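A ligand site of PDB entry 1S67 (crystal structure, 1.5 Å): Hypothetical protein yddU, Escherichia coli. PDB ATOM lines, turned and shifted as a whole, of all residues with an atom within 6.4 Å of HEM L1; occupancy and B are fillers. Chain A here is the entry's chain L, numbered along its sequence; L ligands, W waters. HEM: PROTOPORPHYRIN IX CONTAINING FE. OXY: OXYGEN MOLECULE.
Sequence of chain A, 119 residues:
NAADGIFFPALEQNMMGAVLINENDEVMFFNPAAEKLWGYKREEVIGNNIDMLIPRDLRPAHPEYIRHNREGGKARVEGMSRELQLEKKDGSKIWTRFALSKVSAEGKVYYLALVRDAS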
ATOM      1  N   VAL A  19      -4.603  -7.768  -9.890  1.00  0.00           N
ATOM      2  CA  VAL A  19      -5.074  -6.460  -9.434  1.00  0.00           C
ATOM      3  C   VAL A  19      -5.852  -6.629  -8.133  1.00  0.00           C
ATOM      4  O   VAL A  19      -6.971  -7.142  -8.137  1.00  0.00           O
ATOM      5  CB  VAL A  19      -5.976  -5.783 -10.490  1.00  0.00           C
ATOM      6  CG1 VAL A  19      -6.343  -4.374 -10.064  1.00  0.00           C
ATOM      7  CG2 VAL A  19      -5.284  -5.773 -11.852  1.00  0.00           C
ATOM      8  N   LEU A  20      -5.248  -6.222  -7.022  1.00  0.00           N
ATOM      9  CA  LEU A  20      -5.905  -6.255  -5.719  1.00  0.00           C
ATOM     10  C   LEU A  20      -6.412  -4.868  -5.362  1.00  0.00           C
ATOM     11  O   LEU A  20      -5.730  -3.877  -5.607  1.00  0.00           O
ATOM     12  CB  LEU A  20      -4.939  -6.751  -4.646  1.00  0.00           C
ATOM     13  CG  LEU A  20      -5.532  -7.105  -3.278  1.00  0.00           C
ATOM     14  CD1 LEU A  20      -6.349  -8.384  -3.343  1.00  0.00           C
ATOM     15  CD2 LEU A  20      -4.424  -7.247  -2.252  1.00  0.00           C
ATOM     16  N   ILE A  21      -7.621  -4.798  -4.805  1.00  0.00           N
ATOM     17  CA  ILE A  21      -8.181  -3.548  -4.279  1.00  0.00           C
ATOM     18  C   ILE A  21      -8.607  -3.718  -2.828  1.00  0.00           C
ATOM     19  O   ILE A  21      -9.104  -4.774  -2.443  1.00  0.00           O
ATOM     20  CB  ILE A  21      -9.382  -3.060  -5.154  1.00  0.00           C
ATOM     21  CG1 ILE A  21     -10.478  -4.120  -5.251  1.00  0.00           C
ATOM     22  CG2 ILE A  21      -8.904  -2.680  -6.549  1.00  0.00           C
ATOM     23  CD1 ILE A  21     -11.781  -3.597  -5.831  1.00  0.00           C
ATOM     24  N   TRP A  38      -2.806  -4.022 -19.501  1.00  0.00           N
ATOM     25  CA  TRP A  38      -3.485  -2.729 -19.456  1.00  0.00           C
ATOM     26  C   TRP A  38      -2.667  -1.599 -20.099  1.00  0.00           C
ATOM     27  O   TRP A  38      -3.222  -0.550 -20.436  1.00  0.00           O
ATOM     28  CB  TRP A  38      -3.799  -2.345 -18.000  1.00  0.00           C
ATOM     29  CG  TRP A  38      -5.195  -2.699 -17.582  1.00  0.00           C
ATOM     30  CD1 TRP A  38      -6.340  -2.067 -17.940  1.00  0.00           C
ATOM     31  CD2 TRP A  38      -5.581  -3.769 -16.711  1.00  0.00           C
ATOM     32  NE1 TRP A  38      -7.422  -2.675 -17.356  1.00  0.00           N
ATOM     33  CE2 TRP A  38      -6.982  -3.722 -16.597  1.00  0.00           C
ATOM     34  CE3 TRP A  38      -4.879  -4.766 -16.019  1.00  0.00           C
ATOM     35  CZ2 TRP A  38      -7.704  -4.636 -15.818  1.00  0.00           C
ATOM     36  CZ3 TRP A  38      -5.595  -5.672 -15.251  1.00  0.00           C
ATOM     37  CH2 TRP A  38      -6.992  -5.597 -15.154  1.00  0.00           C
ATOM     38  N   ILE A  50     -10.503   2.056  -8.548  1.00  0.00           N
ATOM     39  CA  ILE A  50     -10.654   0.901  -9.439  1.00  0.00           C
ATOM     40  C   ILE A  50     -11.224   1.275 -10.821  1.00  0.00           C
ATOM     41  O   ILE A  50     -10.980   0.567 -11.803  1.00  0.00           O
ATOM     42  CB  ILE A  50     -11.530  -0.212  -8.781  1.00  0.00           C
ATOM     43  CG1 ILE A  50     -11.601  -1.484  -9.636  1.00  0.00           C
ATOM     44  CG2 ILE A  50     -12.969   0.277  -8.527  1.00  0.00           C
ATOM     45  CD1 ILE A  50     -10.260  -2.055 -10.064  1.00  0.00           C
ATOM     46  N   LEU A  53      -9.169   1.368 -14.271  1.00  0.00           N
ATOM     47  CA  LEU A  53      -8.920   0.111 -14.976  1.00  0.00           C
ATOM     48  C   LEU A  53     -10.160  -0.467 -15.646  1.00  0.00           C
ATOM     49  O   LEU A  53     -10.065  -1.435 -16.393  1.00  0.00           O
ATOM     50  CB  LEU A  53      -8.341  -0.927 -14.002  1.00  0.00           C
ATOM     51  CG  LEU A  53      -7.048  -0.557 -13.275  1.00  0.00           C
ATOM     52  CD1 LEU A  53      -6.699  -1.625 -12.260  1.00  0.00           C
ATOM     53  CD2 LEU A  53      -5.909  -0.352 -14.264  1.00  0.00           C
ATOM     54  N   ILE A  54     -11.330   0.123 -15.390  1.00  0.00           N
ATOM     55  CA  ILE A  54     -12.565  -0.299 -16.044  1.00  0.00           C
ATOM     56  C   ILE A  54     -12.671   0.436 -17.379  1.00  0.00           C
ATOM     57  O   ILE A  54     -12.263   1.598 -17.474  1.00  0.00           O
ATOM     58  CB  ILE A  54     -13.795   0.031 -15.151  1.00  0.00           C
ATOM     59  CG1 ILE A  54     -13.626  -0.551 -13.735  1.00  0.00           C
ATOM     60  CG2 ILE A  54     -15.088  -0.501 -15.776  1.00  0.00           C
ATOM     61  CD1 ILE A  54     -13.424  -2.061 -13.674  1.00  0.00           C
ATOM     62  N   PRO A  55     -13.175  -0.223 -18.427  1.00  0.00           N
ATOM     63  CA  PRO A  55     -13.476   0.458 -19.698  1.00  0.00           C
ATOM     64  C   PRO A  55     -14.451   1.625 -19.513  1.00  0.00           C
ATOM     65  O   PRO A  55     -15.260   1.616 -18.585  1.00  0.00           O
ATOM     66  CB  PRO A  55     -14.109  -0.646 -20.539  1.00  0.00           C
ATOM     67  CG  PRO A  55     -13.575  -1.905 -19.986  1.00  0.00           C
ATOM     68  CD  PRO A  55     -13.445  -1.670 -18.513  1.00  0.00           C
ATOM     69  N   LEU A  58     -18.174   0.796 -19.688  1.00  0.00           N
ATOM     70  CA  LEU A  58     -18.639  -0.013 -18.564  1.00  0.00           C
ATOM     71  C   LEU A  58     -18.483   0.694 -17.217  1.00  0.00           C
ATOM     72  O   LEU A  58     -18.762   0.116 -16.172  1.00  0.00           O
ATOM     73  CB  LEU A  58     -17.873  -1.352 -18.528  1.00  0.00           C
ATOM     74  CG  LEU A  58     -18.607  -2.665 -18.197  1.00  0.00           C
ATOM     75  CD1 LEU A  58     -17.895  -3.410 -17.066  1.00  0.00           C
ATOM     76  CD2 LEU A  58     -20.080  -2.499 -17.850  1.00  0.00           C
ATOM     77  N   HIS A  62     -20.157  -0.340 -13.256  1.00  0.00           N
ATOM     78  CA  HIS A  62     -19.217  -1.113 -12.438  1.00  0.00           C
ATOM     79  C   HIS A  62     -19.159  -0.761 -10.941  1.00  0.00           C
ATOM     80  O   HIS A  62     -18.983  -1.653 -10.119  1.00  0.00           O
ATOM     81  CB  HIS A  62     -17.803  -1.094 -13.023  1.00  0.00           C
ATOM     82  CG  HIS A  62     -16.989  -2.283 -12.634  1.00  0.00           C
ATOM     83  ND1 HIS A  62     -16.180  -2.304 -11.520  1.00  0.00           N
ATOM     84  CD2 HIS A  62     -16.881  -3.519 -13.200  1.00  0.00           C
ATOM     85  CE1 HIS A  62     -15.600  -3.484 -11.422  1.00  0.00           C
ATOM     86  NE2 HIS A  62     -16.010  -4.240 -12.433  1.00  0.00           N
ATOM     87  N   TYR A  65     -21.791  -2.756  -9.232  1.00  0.00           N
ATOM     88  CA  TYR A  65     -21.471  -4.179  -9.128  1.00  0.00           C
ATOM     89  C   TYR A  65     -20.647  -4.474  -7.873  1.00  0.00           C
ATOM     90  O   TYR A  65     -20.896  -5.461  -7.179  1.00  0.00           O
ATOM     91  CB  TYR A  65     -20.692  -4.674 -10.361  1.00  0.00           C
ATOM     92  CG  TYR A  65     -21.421  -4.575 -11.694  1.00  0.00           C
ATOM     93  CD1 TYR A  65     -22.815  -4.651 -11.769  1.00  0.00           C
ATOM     94  CD2 TYR A  65     -20.707  -4.416 -12.881  1.00  0.00           C
ATOM     95  CE1 TYR A  65     -23.464  -4.561 -12.992  1.00  0.00           C
ATOM     96  CE2 TYR A  65     -21.356  -4.326 -14.105  1.00  0.00           C
ATOM     97  CZ  TYR A  65     -22.728  -4.403 -14.159  1.00  0.00           C
ATOM     98  OH  TYR A  65     -23.370  -4.313 -15.371  1.00  0.00           O
ATOM     99  N   ILE A  66     -19.658  -3.620  -7.594  1.00  0.00           N
ATOM    100  CA  ILE A  66     -18.786  -3.770  -6.434  1.00  0.00           C
ATOM    101  C   ILE A  66     -19.545  -3.480  -5.144  1.00  0.00           C
ATOM    102  O   ILE A  66     -19.366  -4.173  -4.144  1.00  0.00           O
ATOM    103  CB  ILE A  66     -17.535  -2.854  -6.542  1.00  0.00           C
ATOM    104  CG1 ILE A  66     -16.677  -3.261  -7.743  1.00  0.00           C
ATOM    105  CG2 ILE A  66     -16.712  -2.909  -5.251  1.00  0.00           C
ATOM    106  CD1 ILE A  66     -15.437  -2.409  -7.950  1.00  0.00           C
ATOM    107  N   HIS A  68     -22.733  -3.810  -4.515  1.00  0.00           N
ATOM    108  CA  HIS A  68     -23.719  -4.857  -4.238  1.00  0.00           C
ATOM    109  C   HIS A  68     -23.087  -6.084  -3.568  1.00  0.00           C
ATOM    110  O   HIS A  68     -23.685  -6.677  -2.674  1.00  0.00           O
ATOM    111  CB  HIS A  68     -24.429  -5.282  -5.525  1.00  0.00           C
ATOM    112  CG  HIS A  68     -25.345  -6.454  -5.359  1.00  0.00           C
ATOM    113  ND1 HIS A  68     -25.158  -7.645  -6.038  1.00  0.00           N
ATOM    114  CD2 HIS A  68     -26.461  -6.620  -4.606  1.00  0.00           C
ATOM    115  CE1 HIS A  68     -26.119  -8.495  -5.691  1.00  0.00           C
ATOM    116  NE2 HIS A  68     -26.921  -7.889  -4.830  1.00  0.00           N
ATOM    117  N   ASN A  69     -21.887  -6.443  -4.005  1.00  0.00           N
ATOM    118  CA  ASN A  69     -21.172  -7.598  -3.466  1.00  0.00           C
ATOM    119  C   ASN A  69     -20.658  -7.353  -2.038  1.00  0.00           C
ATOM    120  O   ASN A  69     -20.525  -8.293  -1.250  1.00  0.00           O
ATOM    121  CB  ASN A  69     -20.012  -7.988  -4.379  1.00  0.00           C
ATOM    122  CG  ASN A  69     -19.548  -9.424  -4.152  1.00  0.00           C
ATOM    123  OD1 ASN A  69     -20.058 -10.354  -4.760  1.00  0.00           O
ATOM    124  ND2 ASN A  69     -18.572  -9.589  -3.265  1.00  0.00           N
ATOM    125  N   GLU A  78     -16.268 -15.786  -3.114  1.00  0.00           N
ATOM    126  CA  GLU A  78     -15.434 -15.292  -4.216  1.00  0.00           C
ATOM    127  C   GLU A  78     -16.199 -14.545  -5.319  1.00  0.00           C
ATOM    128  O   GLU A  78     -16.289 -13.315  -5.292  1.00  0.00           O
ATOM    129  CB  GLU A  78     -14.606 -16.442  -4.803  1.00  0.00           C
ATOM    130  CG  GLU A  78     -13.365 -16.805  -3.996  1.00  0.00           C
ATOM    131  CD  GLU A  78     -13.693 -17.406  -2.636  1.00  0.00           C
ATOM    132  OE1 GLU A  78     -14.268 -18.510  -2.603  1.00  0.00           O
ATOM    133  OE2 GLU A  78     -13.393 -16.765  -1.608  1.00  0.00           O
ATOM    134  N   GLY A  79     -16.742 -15.300  -6.283  1.00  0.00           N
ATOM    135  CA  GLY A  79     -17.496 -14.701  -7.371  1.00  0.00           C
ATOM    136  C   GLY A  79     -17.641 -15.578  -8.597  1.00  0.00           C
ATOM    137  O   GLY A  79     -18.528 -16.435  -8.643  1.00  0.00           O
ATOM    138  N   MET A  80     -16.773 -15.374  -9.586  1.00  0.00           N
ATOM    139  CA  MET A  80     -16.967 -15.966 -10.910  1.00  0.00           C
ATOM    140  C   MET A  80     -15.725 -15.871 -11.803  1.00  0.00           C
ATOM    141  O   MET A  80     -14.783 -15.128 -11.516  1.00  0.00           O
ATOM    142  CB  MET A  80     -18.118 -15.245 -11.607  1.00  0.00           C
ATOM    143  CG  MET A  80     -17.939 -13.733 -11.720  1.00  0.00           C
ATOM    144  SD  MET A  80     -19.458 -12.788 -11.577  1.00  0.00           S
ATOM    145  CE  MET A  80     -20.394 -13.437 -12.947  1.00  0.00           C
ATOM    146  N   ARG A  82     -15.035 -15.417 -16.082  1.00  0.00           N
ATOM    147  CA  ARG A  82     -15.590 -15.205 -17.418  1.00  0.00           C
ATOM    148  C   ARG A  82     -14.677 -14.316 -18.284  1.00  0.00           C
ATOM    149  O   ARG A  82     -13.704 -13.756 -17.793  1.00  0.00           O
ATOM    150  CB  ARG A  82     -16.981 -14.571 -17.324  1.00  0.00           C
ATOM    151  CG  ARG A  82     -17.000 -13.184 -16.691  1.00  0.00           C
ATOM    152  CD  ARG A  82     -17.183 -13.188 -15.184  1.00  0.00           C
ATOM    153  NE  ARG A  82     -17.327 -11.831 -14.653  1.00  0.00           N
ATOM    154  CZ  ARG A  82     -16.445 -11.207 -13.871  1.00  0.00           C
ATOM    155  NH1 ARG A  82     -16.712  -9.972 -13.454  1.00  0.00           N
ATOM    156  NH2 ARG A  82     -15.309 -11.781 -13.492  1.00  0.00           N
ATOM    157  N   LEU A  84     -13.878 -11.019 -20.326  1.00  0.00           N
ATOM    158  CA  LEU A  84     -14.255  -9.592 -20.303  1.00  0.00           C
ATOM    159  C   LEU A  84     -13.378  -8.758 -21.231  1.00  0.00           C
ATOM    160  O   LEU A  84     -12.181  -9.015 -21.344  1.00  0.00           O
ATOM    161  CB  LEU A  84     -14.137  -9.045 -18.883  1.00  0.00           C
ATOM    162  CG  LEU A  84     -14.962  -9.724 -17.789  1.00  0.00           C
ATOM    163  CD1 LEU A  84     -14.515  -9.243 -16.425  1.00  0.00           C
ATOM    164  CD2 LEU A  84     -16.441  -9.471 -17.990  1.00  0.00           C
ATOM    165  N   GLN A  85     -13.972  -7.752 -21.868  1.00  0.00           N
ATOM    166  CA  GLN A  85     -13.241  -6.862 -22.757  1.00  0.00           C
ATOM    167  C   GLN A  85     -12.462  -5.794 -21.978  1.00  0.00           C
ATOM    168  O   GLN A  85     -13.046  -4.833 -21.467  1.00  0.00           O
ATOM    169  CB  GLN A  85     -14.178  -6.204 -23.770  1.00  0.00           C
ATOM    170  CG  GLN A  85     -13.467  -5.634 -24.982  1.00  0.00           C
ATOM    171  CD  GLN A  85     -14.436  -5.067 -26.003  1.00  0.00           C
ATOM    172  OE1 GLN A  85     -15.256  -4.211 -25.689  1.00  0.00           O
ATOM    173  NE2 GLN A  85     -14.333  -5.538 -27.251  1.00  0.00           N
ATOM    174  N   LEU A  86     -11.154  -5.990 -21.869  1.00  0.00           N
ATOM    175  CA  LEU A  86     -10.254  -5.049 -21.212  1.00  0.00           C
ATOM    176  C   LEU A  86      -9.928  -3.871 -22.121  1.00  0.00           C
ATOM    177  O   LEU A  86      -9.639  -4.066 -23.304  1.00  0.00           O
ATOM    178  CB  LEU A  86      -8.962  -5.787 -20.822  1.00  0.00           C
ATOM    179  CG  LEU A  86      -7.952  -5.069 -19.916  1.00  0.00           C
ATOM    180  CD1 LEU A  86      -7.298  -6.074 -18.973  1.00  0.00           C
ATOM    181  CD2 LEU A  86      -6.892  -4.335 -20.725  1.00  0.00           C
ATOM    182  N   GLU A  87      -9.981  -2.659 -21.577  1.00  0.00           N
ATOM    183  CA  GLU A  87      -9.578  -1.454 -22.302  1.00  0.00           C
ATOM    184  C   GLU A  87      -8.228  -0.947 -21.780  1.00  0.00           C
ATOM    185  O   GLU A  87      -8.078  -0.687 -20.590  1.00  0.00           O
ATOM    186  CB  GLU A  87     -10.631  -0.354 -22.173  1.00  0.00           C
ATOM    187  CG  GLU A  87     -10.442   0.795 -23.145  1.00  0.00           C
ATOM    188  CD  GLU A  87     -11.515   1.860 -23.030  1.00  0.00           C
ATOM    189  OE1 GLU A  87     -12.460   1.840 -23.841  1.00  0.00           O
ATOM    190  OE2 GLU A  87     -11.408   2.713 -22.128  1.00  0.00           O
ATOM    191  N   THR A  96     -10.053 -10.936 -22.756  1.00  0.00           N
ATOM    192  CA  THR A  96      -9.257 -11.565 -21.692  1.00  0.00           C
ATOM    193  C   THR A  96     -10.044 -12.653 -20.953  1.00  0.00           C
ATOM    194  O   THR A  96     -11.127 -13.045 -21.391  1.00  0.00           O
ATOM    195  CB  THR A  96      -8.780 -10.474 -20.695  1.00  0.00           C
ATOM    196  OG1 THR A  96      -9.908  -9.749 -20.179  1.00  0.00           O
ATOM    197  CG2 THR A  96      -7.950  -9.402 -21.394  1.00  0.00           C
ATOM    198  N   PHE A  98     -10.856 -13.126 -16.921  1.00  0.00           N
ATOM    199  CA  PHE A  98     -10.783 -12.768 -15.503  1.00  0.00           C
ATOM    200  C   PHE A  98     -11.165 -13.944 -14.613  1.00  0.00           C
ATOM    201  O   PHE A  98     -11.868 -14.871 -15.030  1.00  0.00           O
ATOM    202  CB  PHE A  98     -11.696 -11.575 -15.207  1.00  0.00           C
ATOM    203  CG  PHE A  98     -11.064 -10.234 -15.475  1.00  0.00           C
ATOM    204  CD1 PHE A  98     -10.867  -9.320 -14.452  1.00  0.00           C
ATOM    205  CD2 PHE A  98     -10.652  -9.892 -16.755  1.00  0.00           C
ATOM    206  CE1 PHE A  98     -10.285  -8.090 -14.695  1.00  0.00           C
ATOM    207  CE2 PHE A  98     -10.061  -8.662 -17.003  1.00  0.00           C
ATOM    208  CZ  PHE A  98      -9.873  -7.762 -15.976  1.00  0.00           C
ATOM    209  N   LEU A 100     -12.209 -13.467 -10.835  1.00  0.00           N
ATOM    210  CA  LEU A 100     -12.416 -12.610  -9.670  1.00  0.00           C
ATOM    211  C   LEU A 100     -12.578 -13.418  -8.386  1.00  0.00           C
ATOM    212  O   LEU A 100     -13.215 -14.477  -8.367  1.00  0.00           O
ATOM    213  CB  LEU A 100     -13.650 -11.732  -9.880  1.00  0.00           C
ATOM    214  CG  LEU A 100     -13.942 -10.674  -8.811  1.00  0.00           C
ATOM    215  CD1 LEU A 100     -12.846  -9.614  -8.777  1.00  0.00           C
ATOM    216  CD2 LEU A 100     -15.295 -10.038  -9.049  1.00  0.00           C
ATOM    217  N   SER A 101     -12.007 -12.896  -7.304  1.00  0.00           N
ATOM    218  CA  SER A 101     -12.060 -13.524  -5.979  1.00  0.00           C
ATOM    219  C   SER A 101     -12.343 -12.502  -4.891  1.00  0.00           C
ATOM    220  O   SER A 101     -12.080 -11.306  -5.069  1.00  0.00           O
ATOM    221  CB  SER A 101     -10.747 -14.250  -5.681  1.00  0.00           C
ATOM    222  OG  SER A 101     -10.388 -15.113  -6.751  1.00  0.00           O
ATOM    223  N   TYR A 111     -10.505  -7.617  -3.167  1.00  0.00           N
ATOM    224  CA  TYR A 111     -10.857  -8.341  -4.393  1.00  0.00           C
ATOM    225  C   TYR A 111      -9.636  -8.529  -5.295  1.00  0.00           C
ATOM    226  O   TYR A 111      -9.022  -7.550  -5.711  1.00  0.00           O
ATOM    227  CB  TYR A 111     -11.933  -7.590  -5.186  1.00  0.00           C
ATOM    228  CG  TYR A 111     -13.292  -7.561  -4.525  1.00  0.00           C
ATOM    229  CD1 TYR A 111     -13.790  -6.377  -3.961  1.00  0.00           C
ATOM    230  CD2 TYR A 111     -14.094  -8.697  -4.468  1.00  0.00           C
ATOM    231  CE1 TYR A 111     -15.034  -6.340  -3.361  1.00  0.00           C
ATOM    232  CE2 TYR A 111     -15.350  -8.666  -3.870  1.00  0.00           C
ATOM    233  CZ  TYR A 111     -15.810  -7.478  -3.318  1.00  0.00           C
ATOM    234  OH  TYR A 111     -17.057  -7.433  -2.725  1.00  0.00           O
ATOM    235  N   LEU A 112      -9.285  -9.781  -5.598  1.00  0.00           N
ATOM    236  CA  LEU A 112      -8.168 -10.091  -6.494  1.00  0.00           C
ATOM    237  C   LEU A 112      -8.661 -10.661  -7.827  1.00  0.00           C
ATOM    238  O   LEU A 112      -9.168 -11.785  -7.879  1.00  0.00           O
ATOM    239  CB  LEU A 112      -7.205 -11.086  -5.845  1.00  0.00           C
ATOM    240  CG  LEU A 112      -5.988 -11.500  -6.669  1.00  0.00           C
ATOM    241  CD1 LEU A 112      -5.018 -10.337  -6.839  1.00  0.00           C
ATOM    242  CD2 LEU A 112      -5.276 -12.710  -6.065  1.00  0.00           C
ATOM    243  N   ALA A 113      -8.510  -9.880  -8.898  1.00  0.00           N
ATOM    244  CA  ALA A 113      -8.879 -10.314 -10.246  1.00  0.00           C
ATOM    245  C   ALA A 113      -7.654 -10.834 -11.003  1.00  0.00           C
ATOM    246  O   ALA A 113      -6.762 -10.051 -11.346  1.00  0.00           O
ATOM    247  CB  ALA A 113      -9.516  -9.166 -11.003  1.00  0.00           C
ATOM    248  N   VAL A 115      -6.089 -12.075 -14.325  1.00  0.00           N
ATOM    249  CA  VAL A 115      -6.398 -11.841 -15.735  1.00  0.00           C
ATOM    250  C   VAL A 115      -5.344 -12.488 -16.652  1.00  0.00           C
ATOM    251  O   VAL A 115      -4.172 -12.554 -16.300  1.00  0.00           O
ATOM    252  CB  VAL A 115      -6.445 -10.326 -16.039  1.00  0.00           C
ATOM    253  CG1 VAL A 115      -7.033 -10.057 -17.421  1.00  0.00           C
ATOM    254  CG2 VAL A 115      -7.223  -9.584 -14.956  1.00  0.00           C
HETATM  255  CHA HEM L   1     -18.364  -7.176 -11.512  1.00  0.00           C
HETATM  256  CHB HEM L   1     -16.335  -6.035 -15.774  1.00  0.00           C
HETATM  257  CHC HEM L   1     -12.078  -5.267 -13.575  1.00  0.00           C
HETATM  258  CHD HEM L   1     -14.171  -6.009  -9.258  1.00  0.00           C
HETATM  259  C1A HEM L   1     -18.185  -6.972 -12.855  1.00  0.00           C
HETATM  260  C2A HEM L   1     -19.168  -7.190 -13.888  1.00  0.00           C
HETATM  261  C3A HEM L   1     -18.613  -6.881 -15.069  1.00  0.00           C
HETATM  262  C4A HEM L   1     -17.248  -6.449 -14.829  1.00  0.00           C
HETATM  263  CMA HEM L   1     -19.326  -6.974 -16.437  1.00  0.00           C
HETATM  264  CAA HEM L   1     -20.605  -7.699 -13.659  1.00  0.00           C
HETATM  265  CBA HEM L   1     -20.617  -9.219 -13.444  1.00  0.00           C
HETATM  266  CGA HEM L   1     -21.068  -9.967 -14.682  1.00  0.00           C
HETATM  267  O1A HEM L   1     -21.971  -9.485 -15.403  1.00  0.00           O
HETATM  268  O2A HEM L   1     -20.526 -11.072 -14.939  1.00  0.00           O
HETATM  269  C1B HEM L   1     -15.020  -5.699 -15.556  1.00  0.00           C
HETATM  270  C2B HEM L   1     -14.081  -5.202 -16.546  1.00  0.00           C
HETATM  271  C3B HEM L   1     -12.904  -4.997 -15.936  1.00  0.00           C
HETATM  272  C4B HEM L   1     -13.060  -5.336 -14.536  1.00  0.00           C
HETATM  273  CMB HEM L   1     -14.392  -4.975 -18.043  1.00  0.00           C
HETATM  274  CAB HEM L   1     -11.606  -4.478 -16.596  1.00  0.00           C
HETATM  275  CBB HEM L   1     -11.075  -5.144 -17.618  1.00  0.00           C
HETATM  276  C1C HEM L   1     -12.250  -5.458 -12.220  1.00  0.00           C
HETATM  277  C2C HEM L   1     -11.205  -5.491 -11.216  1.00  0.00           C
HETATM  278  C3C HEM L   1     -11.793  -5.691 -10.023  1.00  0.00           C
HETATM  279  C4C HEM L   1     -13.218  -5.802 -10.236  1.00  0.00           C
HETATM  280  CMC HEM L   1      -9.695  -5.311 -11.489  1.00  0.00           C
HETATM  281  CAC HEM L   1     -11.108  -5.795  -8.644  1.00  0.00           C
HETATM  282  CBC HEM L   1      -9.944  -6.444  -8.504  1.00  0.00           C
HETATM  283  C1D HEM L   1     -15.461  -6.445  -9.442  1.00  0.00           C
HETATM  284  C2D HEM L   1     -16.344  -6.909  -8.393  1.00  0.00           C
HETATM  285  C3D HEM L   1     -17.660  -7.270  -9.100  1.00  0.00           C
HETATM  286  C4D HEM L   1     -17.441  -6.991 -10.503  1.00  0.00           C
HETATM  287  CMD HEM L   1     -16.037  -7.021  -6.892  1.00  0.00           C
HETATM  288  CAD HEM L   1     -18.946  -7.825  -8.455  1.00  0.00           C
HETATM  289  CBD HEM L   1     -19.090  -9.308  -8.770  1.00  0.00           C
HETATM  290  CGD HEM L   1     -20.536  -9.720  -8.695  1.00  0.00           C
HETATM  291  O1D HEM L   1     -21.183  -9.820  -9.769  1.00  0.00           O
HETATM  292  O2D HEM L   1     -21.047  -9.932  -7.568  1.00  0.00           O
HETATM  293  NA  HEM L   1     -17.023  -6.509 -13.467  1.00  0.00           N
HETATM  294  NB  HEM L   1     -14.361  -5.761 -14.337  1.00  0.00           N
HETATM  295  NC  HEM L   1     -13.468  -5.648 -11.591  1.00  0.00           N
HETATM  296  ND  HEM L   1     -16.138  -6.502 -10.661  1.00  0.00           N
HETATM  297 FE   HEM L   1     -15.292  -5.959 -12.490  1.00  0.00          FE
HETATM  298  O1  OXY L   2     -14.547  -8.340 -12.643  1.00  0.00           O
HETATM  299  O2  OXY L   2     -13.835  -9.147 -12.739  1.00  0.00           O
HETATM  300  O   HOH W   1     -22.758  -7.375  -7.882  1.00  0.00           O
HETATM  301  O   HOH W   2     -23.104 -10.835 -11.438  1.00  0.00           O
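An oxygen (O2) of OXY L2 is in hydrogen-bond range of the guanidinium group of Arg 82 (3.1 Å). O2D of HEM L1 sits close to OD1 of Asn 69 (3.0 Å). A ring nitrogen (NE2) of His 62 binds an iron atom (FE) of HEM L1, at 1.9 Å. The guanidinium group (NE) of Arg 82 lies within salt-bridge range of an oxygen (O2A) of HEM L1, 3.3 Å away.
An oxygen (O1) of OXY L2 is bound to an iron atom (FE) of HEM L1 (2.5 Å).
N of Ala 113 lies within hydrogen-bond range of O of Val 19. O of Arg 82 lies within hydrogen-bond range of N of Phe 98, at 3.0 Å. O of Leu 53 sits at hydrogen-bond distance from NE1 of Trp 38 (3.1 Å). The backbone NH (N) of Leu 100 sits at hydrogen-bond distance from the backbone carbonyl oxygen (O) of Met 80. The backbone carbonyl oxygen (O) of Leu 84 sits at hydrogen-bond distance from the side-chain hydroxyl (OG1) of Thr 96 (2.7 Å). The side-chain hydroxyl of Tyr 111 is in hydrogen-bond range of the side-chain amide nitrogen of Asn 69, 2.7 Å away. The backbone carbonyl oxygen (O) of Tyr 111 sits at hydrogen-bond distance from the backbone NH (N) of Ile 21, at 3.2 Å.
Val 19 touches HEM L1 (O to CBC, 3.1 Å). Ile 21 touches HEM L1 (CD1 to CAC, 3.6 Å). Trp 38 touches HEM L1. CD1 of Ile 50 touches CMC of HEM L1 (3.6 Å). Leu 53 touches HEM L1 (O to CAB, 3.4 Å). CD1 of Ile 54 touches C4B of HEM L1 (3.4 Å). CD of Pro 55 touches CMB of HEM L1, at 3.5 Å. CD1 of Leu 58 touches CHB of HEM L1, at 3.3 Å. Tyr 65 touches HEM L1. Ile 66 touches HEM L1. Met 80 touches HEM L1 (CE to O2A, 3.1 Å). Leu 84 touches HEM L1. O of Gln 85 touches CMB of HEM L1 (3.7 Å). CA of Leu 86 touches CBB of HEM L1 (3.7 Å). Phe 98 touches HEM L1. Leu 100 touches HEM L1 (CD2 to C2D, 3.4 Å). Tyr 111 touches HEM L1 (O to CBC, 3.1 Å). Ala 113 touches HEM L1. Of the 30 residues printed, 21 come within 4 Å of HEM L1.
Water W1 lies within hydrogen-bond range of O of Tyr 65 (2.8 Å), ND1 of His 68 (3.0 Å) and O2D of HEM L1 (3.1 Å).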
